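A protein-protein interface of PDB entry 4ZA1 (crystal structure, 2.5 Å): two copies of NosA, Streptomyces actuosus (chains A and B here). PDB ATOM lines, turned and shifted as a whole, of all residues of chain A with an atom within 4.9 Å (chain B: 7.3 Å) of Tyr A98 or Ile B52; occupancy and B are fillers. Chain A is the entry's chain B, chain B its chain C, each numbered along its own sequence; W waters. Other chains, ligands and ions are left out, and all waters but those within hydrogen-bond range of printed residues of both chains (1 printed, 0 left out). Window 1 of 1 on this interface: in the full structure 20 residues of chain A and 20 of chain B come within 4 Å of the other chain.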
ATOM      1  N   LEU A   9     -19.023 -15.174  13.826  1.00  0.00           N
ATOM      2  CA  LEU A   9     -18.044 -15.720  12.884  1.00  0.00           C
ATOM      3  C   LEU A   9     -16.603 -15.393  13.282  1.00  0.00           C
ATOM      4  O   LEU A   9     -16.350 -14.427  14.005  1.00  0.00           O
ATOM      5  CB  LEU A   9     -18.333 -15.234  11.454  1.00  0.00           C
ATOM      6  CG  LEU A   9     -19.718 -15.514  10.846  1.00  0.00           C
ATOM      7  CD1 LEU A   9     -19.915 -14.730   9.553  1.00  0.00           C
ATOM      8  CD2 LEU A   9     -19.953 -17.001  10.609  1.00  0.00           C
ATOM      9  N   TYR A  10     -15.667 -16.213  12.809  1.00  0.00           N
ATOM     10  CA  TYR A  10     -14.245 -16.016  13.086  1.00  0.00           C
ATOM     11  C   TYR A  10     -13.435 -15.970  11.796  1.00  0.00           C
ATOM     12  O   TYR A  10     -13.780 -16.622  10.807  1.00  0.00           O
ATOM     13  CB  TYR A  10     -13.721 -17.099  14.035  1.00  0.00           C
ATOM     14  CG  TYR A  10     -14.467 -17.125  15.354  1.00  0.00           C
ATOM     15  CD1 TYR A  10     -15.654 -17.855  15.496  1.00  0.00           C
ATOM     16  CD2 TYR A  10     -14.007 -16.395  16.451  1.00  0.00           C
ATOM     17  CE1 TYR A  10     -16.352 -17.861  16.693  1.00  0.00           C
ATOM     18  CE2 TYR A  10     -14.698 -16.402  17.654  1.00  0.00           C
ATOM     19  CZ  TYR A  10     -15.868 -17.137  17.768  1.00  0.00           C
ATOM     20  OH  TYR A  10     -16.554 -17.148  18.960  1.00  0.00           O
ATOM     21  N   CYS A  11     -12.362 -15.184  11.815  1.00  0.00           N
ATOM     22  CA  CYS A  11     -11.528 -14.984  10.639  1.00  0.00           C
ATOM     23  C   CYS A  11     -10.062 -15.284  10.941  1.00  0.00           C
ATOM     24  O   CYS A  11      -9.456 -14.656  11.811  1.00  0.00           O
ATOM     25  CB  CYS A  11     -11.687 -13.555  10.110  1.00  0.00           C
ATOM     26  SG  CYS A  11     -10.562 -13.124   8.765  1.00  0.00           S
ATOM     27  N   VAL A  13      -6.183 -15.651   9.221  1.00  0.00           N
ATOM     28  CA  VAL A  13      -5.360 -15.305   8.075  1.00  0.00           C
ATOM     29  C   VAL A  13      -3.970 -15.907   8.228  1.00  0.00           C
ATOM     30  O   VAL A  13      -3.332 -15.815   9.282  1.00  0.00           O
ATOM     31  CB  VAL A  13      -5.362 -13.781   7.768  1.00  0.00           C
ATOM     32  CG1 VAL A  13      -5.647 -12.960   9.011  1.00  0.00           C
ATOM     33  CG2 VAL A  13      -4.076 -13.325   7.085  1.00  0.00           C
ATOM     34  N   ARG A  96      -2.723 -14.896  12.021  1.00  0.00           N
ATOM     35  CA  ARG A  96      -3.547 -13.988  12.817  1.00  0.00           C
ATOM     36  C   ARG A  96      -4.968 -14.524  12.998  1.00  0.00           C
ATOM     37  O   ARG A  96      -5.490 -15.239  12.136  1.00  0.00           O
ATOM     38  CB  ARG A  96      -3.576 -12.599  12.186  1.00  0.00           C
ATOM     39  CG  ARG A  96      -2.349 -11.757  12.489  1.00  0.00           C
ATOM     40  CD  ARG A  96      -1.919 -10.989  11.252  1.00  0.00           C
ATOM     41  NE  ARG A  96      -1.321  -9.702  11.592  1.00  0.00           N
ATOM     42  CZ  ARG A  96      -0.508  -9.013  10.795  1.00  0.00           C
ATOM     43  NH1 ARG A  96      -0.022  -7.848  11.199  1.00  0.00           N
ATOM     44  NH2 ARG A  96      -0.171  -9.485   9.600  1.00  0.00           N
ATOM     45  N   TYR A  97      -5.581 -14.172  14.127  1.00  0.00           N
ATOM     46  CA  TYR A  97      -6.878 -14.717  14.517  1.00  0.00           C
ATOM     47  C   TYR A  97      -7.824 -13.603  14.958  1.00  0.00           C
ATOM     48  O   TYR A  97      -7.487 -12.793  15.822  1.00  0.00           O
ATOM     49  CB  TYR A  97      -6.693 -15.762  15.624  1.00  0.00           C
ATOM     50  CG  TYR A  97      -5.743 -16.870  15.227  1.00  0.00           C
ATOM     51  CD1 TYR A  97      -4.364 -16.754  15.444  1.00  0.00           C
ATOM     52  CD2 TYR A  97      -6.217 -18.022  14.605  1.00  0.00           C
ATOM     53  CE1 TYR A  97      -3.489 -17.760  15.058  1.00  0.00           C
ATOM     54  CE2 TYR A  97      -5.353 -19.037  14.222  1.00  0.00           C
ATOM     55  CZ  TYR A  97      -3.990 -18.901  14.448  1.00  0.00           C
ATOM     56  OH  TYR A  97      -3.140 -19.911  14.057  1.00  0.00           O
ATOM     57  N   TYR A  98      -9.007 -13.562  14.356  1.00  0.00           N
ATOM     58  CA  TYR A  98      -9.956 -12.487  14.627  1.00  0.00           C
ATOM     59  C   TYR A  98     -11.370 -12.988  14.869  1.00  0.00           C
ATOM     60  O   TYR A  98     -11.780 -14.013  14.323  1.00  0.00           O
ATOM     61  CB  TYR A  98     -10.005 -11.501  13.456  1.00  0.00           C
ATOM     62  CG  TYR A  98      -8.690 -10.863  13.076  1.00  0.00           C
ATOM     63  CD1 TYR A  98      -8.139  -9.834  13.844  1.00  0.00           C
ATOM     64  CD2 TYR A  98      -8.014 -11.261  11.924  1.00  0.00           C
ATOM     65  CE1 TYR A  98      -6.940  -9.237  13.486  1.00  0.00           C
ATOM     66  CE2 TYR A  98      -6.817 -10.668  11.556  1.00  0.00           C
ATOM     67  CZ  TYR A  98      -6.285  -9.659  12.338  1.00  0.00           C
ATOM     68  OH  TYR A  98      -5.102  -9.076  11.967  1.00  0.00           O
ATOM     69  N   SER A  99     -12.110 -12.247  15.687  1.00  0.00           N
ATOM     70  CA  SER A  99     -13.557 -12.387  15.750  1.00  0.00           C
ATOM     71  C   SER A  99     -14.184 -11.381  14.794  1.00  0.00           C
ATOM     72  O   SER A  99     -13.796 -10.206  14.766  1.00  0.00           O
ATOM     73  CB  SER A  99     -14.068 -12.151  17.167  1.00  0.00           C
ATOM     74  OG  SER A  99     -13.501 -13.096  18.064  1.00  0.00           O
ATOM     75  N   VAL A 100     -15.141 -11.849  13.999  1.00  0.00           N
ATOM     76  CA  VAL A 100     -15.919 -10.964  13.145  1.00  0.00           C
ATOM     77  C   VAL A 100     -16.982 -10.291  14.003  1.00  0.00           C
ATOM     78  O   VAL A 100     -17.765 -10.963  14.674  1.00  0.00           O
ATOM     79  CB  VAL A 100     -16.546 -11.719  11.954  1.00  0.00           C
ATOM     80  CG1 VAL A 100     -17.481 -10.813  11.157  1.00  0.00           C
ATOM     81  CG2 VAL A 100     -15.447 -12.287  11.058  1.00  0.00           C
ATOM     82  N   GLU A 101     -16.979  -8.963  13.991  1.00  0.00           N
ATOM     83  CA  GLU A 101     -17.907  -8.171  14.792  1.00  0.00           C
ATOM     84  C   GLU A 101     -19.151  -7.773  13.996  1.00  0.00           C
ATOM     85  O   GLU A 101     -20.271  -7.865  14.502  1.00  0.00           O
ATOM     86  CB  GLU A 101     -17.200  -6.937  15.366  1.00  0.00           C
ATOM     87  CG  GLU A 101     -15.965  -7.251  16.208  1.00  0.00           C
ATOM     88  CD  GLU A 101     -16.276  -8.004  17.495  1.00  0.00           C
ATOM     89  OE1 GLU A 101     -17.362  -7.792  18.079  1.00  0.00           O
ATOM     90  OE2 GLU A 101     -15.423  -8.810  17.932  1.00  0.00           O
ATOM     91  N   VAL B  13      -6.737  -3.369   4.957  1.00  0.00           N
ATOM     92  CA  VAL B  13      -6.938  -3.772   6.338  1.00  0.00           C
ATOM     93  C   VAL B  13      -6.394  -2.662   7.221  1.00  0.00           C
ATOM     94  O   VAL B  13      -5.259  -2.217   7.047  1.00  0.00           O
ATOM     95  CB  VAL B  13      -6.243  -5.125   6.645  1.00  0.00           C
ATOM     96  CG1 VAL B  13      -6.422  -5.510   8.104  1.00  0.00           C
ATOM     97  CG2 VAL B  13      -6.790  -6.228   5.746  1.00  0.00           C
ATOM     98  N   VAL B  14      -7.217  -2.208   8.156  1.00  0.00           N
ATOM     99  CA  VAL B  14      -6.850  -1.105   9.030  1.00  0.00           C
ATOM    100  C   VAL B  14      -6.977  -1.559  10.481  1.00  0.00           C
ATOM    101  O   VAL B  14      -8.032  -2.040  10.893  1.00  0.00           O
ATOM    102  CB  VAL B  14      -7.704   0.151   8.720  1.00  0.00           C
ATOM    103  CG1 VAL B  14      -9.071   0.097   9.394  1.00  0.00           C
ATOM    104  CG2 VAL B  14      -6.960   1.410   9.114  1.00  0.00           C
ATOM    105  N   LEU B  15      -5.894  -1.430  11.245  1.00  0.00           N
ATOM    106  CA  LEU B  15      -5.855  -1.967  12.606  1.00  0.00           C
ATOM    107  C   LEU B  15      -5.401  -0.958  13.652  1.00  0.00           C
ATOM    108  O   LEU B  15      -4.486  -0.167  13.414  1.00  0.00           O
ATOM    109  CB  LEU B  15      -4.971  -3.224  12.669  1.00  0.00           C
ATOM    110  CG  LEU B  15      -5.432  -4.449  11.863  1.00  0.00           C
ATOM    111  CD1 LEU B  15      -4.289  -5.425  11.638  1.00  0.00           C
ATOM    112  CD2 LEU B  15      -6.610  -5.154  12.520  1.00  0.00           C
ATOM    113  N   TRP B  16      -6.064  -0.993  14.806  1.00  0.00           N
ATOM    114  CA  TRP B  16      -5.644  -0.235  15.976  1.00  0.00           C
ATOM    115  C   TRP B  16      -5.230  -1.177  17.062  1.00  0.00           C
ATOM    116  O   TRP B  16      -5.965  -2.111  17.396  1.00  0.00           O
ATOM    117  CB  TRP B  16      -6.776   0.623  16.520  1.00  0.00           C
ATOM    118  CG  TRP B  16      -7.261   1.731  15.621  1.00  0.00           C
ATOM    119  CD1 TRP B  16      -6.929   3.080  15.683  1.00  0.00           C
ATOM    120  CD2 TRP B  16      -8.230   1.625  14.526  1.00  0.00           C
ATOM    121  NE1 TRP B  16      -7.593   3.792  14.719  1.00  0.00           N
ATOM    122  CE2 TRP B  16      -8.388   2.981  13.987  1.00  0.00           C
ATOM    123  CE3 TRP B  16      -8.948   0.580  13.949  1.00  0.00           C
ATOM    124  CZ2 TRP B  16      -9.231   3.253  12.920  1.00  0.00           C
ATOM    125  CZ3 TRP B  16      -9.798   0.869  12.876  1.00  0.00           C
ATOM    126  CH2 TRP B  16      -9.933   2.174  12.374  1.00  0.00           C
ATOM    127  N   VAL B  25     -12.141  -3.804  23.334  1.00  0.00           N
ATOM    128  CA  VAL B  25     -13.003  -4.559  22.419  1.00  0.00           C
ATOM    129  C   VAL B  25     -14.462  -4.520  22.887  1.00  0.00           C
ATOM    130  O   VAL B  25     -15.378  -4.405  22.070  1.00  0.00           O
ATOM    131  CB  VAL B  25     -12.519  -6.021  22.261  1.00  0.00           C
ATOM    132  CG1 VAL B  25     -13.518  -6.853  21.463  1.00  0.00           C
ATOM    133  CG2 VAL B  25     -11.150  -6.057  21.596  1.00  0.00           C
ATOM    134  N   THR B  50     -15.964  -5.159   6.801  1.00  0.00           N
ATOM    135  CA  THR B  50     -16.064  -6.047   7.950  1.00  0.00           C
ATOM    136  C   THR B  50     -15.281  -5.491   9.129  1.00  0.00           C
ATOM    137  O   THR B  50     -14.108  -5.145   8.994  1.00  0.00           O
ATOM    138  CB  THR B  50     -15.567  -7.470   7.607  1.00  0.00           C
ATOM    139  OG1 THR B  50     -16.288  -7.972   6.476  1.00  0.00           O
ATOM    140  CG2 THR B  50     -15.768  -8.423   8.784  1.00  0.00           C
ATOM    141  N   TRP B  51     -15.949  -5.396  10.275  1.00  0.00           N
ATOM    142  CA  TRP B  51     -15.300  -5.057  11.537  1.00  0.00           C
ATOM    143  C   TRP B  51     -14.765  -6.305  12.178  1.00  0.00           C
ATOM    144  O   TRP B  51     -15.458  -7.323  12.254  1.00  0.00           O
ATOM    145  CB  TRP B  51     -16.276  -4.351  12.474  1.00  0.00           C
ATOM    146  CG  TRP B  51     -16.695  -2.987  11.979  1.00  0.00           C
ATOM    147  CD1 TRP B  51     -17.921  -2.624  11.423  1.00  0.00           C
ATOM    148  CD2 TRP B  51     -15.889  -1.757  11.961  1.00  0.00           C
ATOM    149  NE1 TRP B  51     -17.928  -1.294  11.082  1.00  0.00           N
ATOM    150  CE2 TRP B  51     -16.740  -0.716  11.378  1.00  0.00           C
ATOM    151  CE3 TRP B  51     -14.596  -1.427  12.359  1.00  0.00           C
ATOM    152  CZ2 TRP B  51     -16.296   0.590  11.213  1.00  0.00           C
ATOM    153  CZ3 TRP B  51     -14.157  -0.109  12.185  1.00  0.00           C
ATOM    154  CH2 TRP B  51     -14.989   0.874  11.624  1.00  0.00           C
ATOM    155  N   ILE B  52     -13.517  -6.241  12.633  1.00  0.00           N
ATOM    156  CA  ILE B  52     -12.859  -7.382  13.256  1.00  0.00           C
ATOM    157  C   ILE B  52     -12.219  -6.978  14.578  1.00  0.00           C
ATOM    158  O   ILE B  52     -11.988  -5.790  14.823  1.00  0.00           O
ATOM    159  CB  ILE B  52     -11.788  -8.011  12.333  1.00  0.00           C
ATOM    160  CG1 ILE B  52     -10.746  -6.965  11.905  1.00  0.00           C
ATOM    161  CG2 ILE B  52     -12.447  -8.680  11.133  1.00  0.00           C
ATOM    162  CD1 ILE B  52      -9.505  -7.536  11.237  1.00  0.00           C
ATOM    163  N   SER B  53     -11.941  -7.971  15.423  1.00  0.00           N
ATOM    164  CA  SER B  53     -11.267  -7.743  16.697  1.00  0.00           C
ATOM    165  C   SER B  53     -10.403  -8.939  17.072  1.00  0.00           C
ATOM    166  O   SER B  53     -10.597 -10.037  16.548  1.00  0.00           O
ATOM    167  CB  SER B  53     -12.286  -7.462  17.808  1.00  0.00           C
ATOM    168  OG  SER B  53     -12.907  -8.656  18.262  1.00  0.00           O
ATOM    169  N   SER B  54      -9.448  -8.718  17.974  1.00  0.00           N
ATOM    170  CA  SER B  54      -8.656  -9.809  18.542  1.00  0.00           C
ATOM    171  C   SER B  54      -8.263  -9.556  19.994  1.00  0.00           C
ATOM    172  O   SER B  54      -7.867  -8.448  20.359  1.00  0.00           O
ATOM    173  CB  SER B  54      -7.410 -10.099  17.695  1.00  0.00           C
ATOM    174  OG  SER B  54      -6.566  -8.969  17.610  1.00  0.00           O
ATOM    175  N   THR B  55      -8.393 -10.596  20.814  1.00  0.00           N
ATOM    176  CA  THR B  55      -7.920 -10.570  22.194  1.00  0.00           C
ATOM    177  C   THR B  55      -6.852 -11.639  22.389  1.00  0.00           C
ATOM    178  O   THR B  55      -6.888 -12.693  21.753  1.00  0.00           O
ATOM    179  CB  THR B  55      -9.052 -10.822  23.216  1.00  0.00           C
ATOM    180  OG1 THR B  55      -9.676 -12.083  22.941  1.00  0.00           O
ATOM    181  CG2 THR B  55     -10.097  -9.704  23.176  1.00  0.00           C
ATOM    182  N   GLN B  61      -6.986  -5.732  19.905  1.00  0.00           N
ATOM    183  CA  GLN B  61      -6.939  -5.075  18.596  1.00  0.00           C
ATOM    184  C   GLN B  61      -8.318  -4.885  17.988  1.00  0.00           C
ATOM    185  O   GLN B  61      -9.168  -5.774  18.059  1.00  0.00           O
ATOM    186  CB  GLN B  61      -6.083  -5.868  17.610  1.00  0.00           C
ATOM    187  CG  GLN B  61      -4.602  -5.546  17.651  1.00  0.00           C
ATOM    188  CD  GLN B  61      -3.829  -6.269  16.564  1.00  0.00           C
ATOM    189  OE1 GLN B  61      -3.987  -7.477  16.366  1.00  0.00           O
ATOM    190  NE2 GLN B  61      -2.988  -5.531  15.849  1.00  0.00           N
ATOM    191  N   TRP B  62      -8.520  -3.721  17.379  1.00  0.00           N
ATOM    192  CA  TRP B  62      -9.726  -3.434  16.616  1.00  0.00           C
ATOM    193  C   TRP B  62      -9.341  -3.113  15.203  1.00  0.00           C
ATOM    194  O   TRP B  62      -8.269  -2.554  14.955  1.00  0.00           O
ATOM    195  CB  TRP B  62     -10.485  -2.274  17.243  1.00  0.00           C
ATOM    196  CG  TRP B  62     -11.898  -2.117  16.733  1.00  0.00           C
ATOM    197  CD1 TRP B  62     -12.359  -1.220  15.775  1.00  0.00           C
ATOM    198  CD2 TRP B  62     -13.088  -2.876  17.146  1.00  0.00           C
ATOM    199  NE1 TRP B  62     -13.707  -1.368  15.573  1.00  0.00           N
ATOM    200  CE2 TRP B  62     -14.206  -2.342  16.363  1.00  0.00           C
ATOM    201  CE3 TRP B  62     -13.329  -3.903  18.051  1.00  0.00           C
ATOM    202  CZ2 TRP B  62     -15.499  -2.831  16.498  1.00  0.00           C
ATOM    203  CZ3 TRP B  62     -14.637  -4.389  18.177  1.00  0.00           C
ATOM    204  CH2 TRP B  62     -15.693  -3.864  17.419  1.00  0.00           C
ATOM    205  N   GLY B  63     -10.204  -3.465  14.256  1.00  0.00           N
ATOM    206  CA  GLY B  63      -9.896  -3.245  12.853  1.00  0.00           C
ATOM    207  C   GLY B  63     -11.068  -3.300  11.899  1.00  0.00           C
ATOM    208  O   GLY B  63     -12.202  -3.576  12.297  1.00  0.00           O
ATOM    209  N   ALA B  64     -10.780  -3.028  10.628  1.00  0.00           N
ATOM    210  CA  ALA B  64     -11.768  -3.110   9.563  1.00  0.00           C
ATOM    211  C   ALA B  64     -11.144  -3.660   8.287  1.00  0.00           C
ATOM    212  O   ALA B  64     -10.012  -3.312   7.936  1.00  0.00           O
ATOM    213  CB  ALA B  64     -12.399  -1.750   9.308  1.00  0.00           C
ATOM    214  N   VAL B  65     -11.887  -4.530   7.607  1.00  0.00           N
ATOM    215  CA  VAL B  65     -11.446  -5.122   6.349  1.00  0.00           C
ATOM    216  C   VAL B  65     -12.353  -4.646   5.216  1.00  0.00           C
ATOM    217  O   VAL B  65     -13.569  -4.860   5.251  1.00  0.00           O
ATOM    218  CB  VAL B  65     -11.450  -6.663   6.408  1.00  0.00           C
ATOM    219  CG1 VAL B  65     -10.848  -7.245   5.133  1.00  0.00           C
ATOM    220  CG2 VAL B  65     -10.691  -7.157   7.633  1.00  0.00           C
ATOM    221  N   GLU B  94      -1.768   0.178  12.283  1.00  0.00           N
ATOM    222  CA  GLU B  94      -1.366  -0.630  11.137  1.00  0.00           C
ATOM    223  C   GLU B  94      -2.339  -0.529   9.967  1.00  0.00           C
ATOM    224  O   GLU B  94      -3.559  -0.490  10.153  1.00  0.00           O
ATOM    225  CB  GLU B  94      -1.194  -2.090  11.552  1.00  0.00           C
ATOM    226  CG  GLU B  94      -0.476  -2.947  10.524  1.00  0.00           C
ATOM    227  CD  GLU B  94      -0.164  -4.341  11.030  1.00  0.00           C
ATOM    228  OE1 GLU B  94      -0.042  -4.521  12.263  1.00  0.00           O
ATOM    229  OE2 GLU B  94      -0.034  -5.257  10.187  1.00  0.00           O
ATOM    230  N   ARG B  96      -2.635  -2.336   5.950  1.00  0.00           N
ATOM    231  CA  ARG B  96      -2.112  -3.235   4.911  1.00  0.00           C
ATOM    232  C   ARG B  96      -2.980  -3.270   3.651  1.00  0.00           C
ATOM    233  O   ARG B  96      -4.193  -3.046   3.707  1.00  0.00           O
ATOM    234  CB  ARG B  96      -1.886  -4.649   5.467  1.00  0.00           C
ATOM    235  CG  ARG B  96      -0.656  -4.762   6.361  1.00  0.00           C
ATOM    236  CD  ARG B  96      -0.488  -6.147   6.974  1.00  0.00           C
ATOM    237  NE  ARG B  96      -1.337  -6.351   8.152  1.00  0.00           N
ATOM    238  CZ  ARG B  96      -2.125  -7.409   8.358  1.00  0.00           C
ATOM    239  NH1 ARG B  96      -2.183  -8.404   7.480  1.00  0.00           N
ATOM    240  NH2 ARG B  96      -2.851  -7.486   9.467  1.00  0.00           N
HETATM  241  O   HOH W   1      -8.658 -12.934  18.826  1.00  0.00           O
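Among the printed residues, pairs that only touch across the chains: Tyr A98 with Ser B53 (3.2 Å), Tyr A97 with Ser B54 (3.3 Å), Ser A99 with Ile B52 (3.3 Å), Glu A101 with Trp B62 (3.6 Å), Tyr A98 with Arg B96 (3.7 Å), Tyr A98 with Ile B52 (3.7 Å), Tyr A98 with Leu B15 (3.8 Å), Val A100 with Trp B51 (3.8 Å), Val A100 with Thr B50 (3.8 Å) and Tyr A98 with Ser B54 (3.9 Å).
Arg B96 touches its own counterpart, Arg A96. Positions printed for both chains: 13 and 96. Of the 15 pairs that touch across the chains among the printed residues, 1 has its exchanged pair printed and touching as well.
The backbone carbonyl oxygen of Cys A11 sits at hydrogen-bond distance from the backbone NH of Tyr A98. The backbone carbonyl oxygen of Val A13 is in hydrogen-bond range of the backbone NH of Arg A96. The backbone carbonyl oxygen (O) of Ser B54 sits at hydrogen-bond distance from the backbone NH (N) of Gln B61 (2.9 Å). N of Leu B15 lies within hydrogen-bond range of O of Glu B94. The backbone NH (N) of Gly B63 sits at hydrogen-bond distance from the backbone carbonyl oxygen (O) of Ile B52, 3.0 Å away. The backbone carbonyl oxygen of Thr B50 is in hydrogen-bond range of the backbone NH of Val B65, at 2.7 Å.
Cys A11 touches none of the printed residues of chain B. Of chain B, only Leu B15 (3.8 Å), Ile B52 (3.7 Å), Ser B53 (3.2 Å), Ser B54 (3.9 Å) and Arg B96 (3.7 Å) come within 4 Å of Tyr A98. Of the printed residues of chain A, Leu B15 touches Tyr A98. Printed residues of chain A within 4 Å of Trp B51: Val A100 and Glu A101. Ile B52 touches two residues of chain A. The nearest residue of chain B that does not touch Tyr A98 is Gln B61 (4.5 Å). The nearest residue of chain A that does not touch Ile B52 is Glu A101 (4.1 Å). The nearest printed residue of chain B that does not touch Tyr A97 is Ser B53 (4.2 Å).
Water W1 lies within hydrogen-bond range of the backbone NH (N) of Thr B55 and the backbone carbonyl oxygen (O) of Tyr A97.
The side-chain hydroxyl (OG) of Ser B53 sits at hydrogen-bond distance from the side-chain carboxylate (OE2) of Glu A101. The guanidinium group of Arg A96 lies within salt-bridge range of the side-chain carboxylate of Glu B94 (2.8 Å). The guanidinium group (NH2) of Arg A96 lies close to the guanidinium group (NH1) of Arg B96, 3.1 Å away. N of Glu A101 sits at hydrogen-bond distance from O of Trp B51 (2.8 Å). N of Ser A99 is in hydrogen-bond range of O of Ser B53 (2.8 Å).
Printed residues of chain B that touch a printed residue of chain A: Leu B15, Thr B50, Trp B51, Ile B52, Ser B53, Ser B54, Trp B62, Glu B94 and Arg B96. Hydrophobic or aromatic side chains of chain B within 4 Å of the printed part of chain A: Leu B15, Trp B51, Ile B52 and Trp B62. Of the 10 printed residues of chain A, 6 touch a printed residue of chain B. Printed residues of chain A that touch a printed residue of chain B: Arg A96, Tyr A97, Tyr A98, Ser A99, Val A100 and Glu A101. Among the printed residues, Asp or Glu carboxylates within 4 Å of a Lys or Arg side-chain nitrogen of the other chain: Arg A96 with Glu B94 (2.8 Å).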
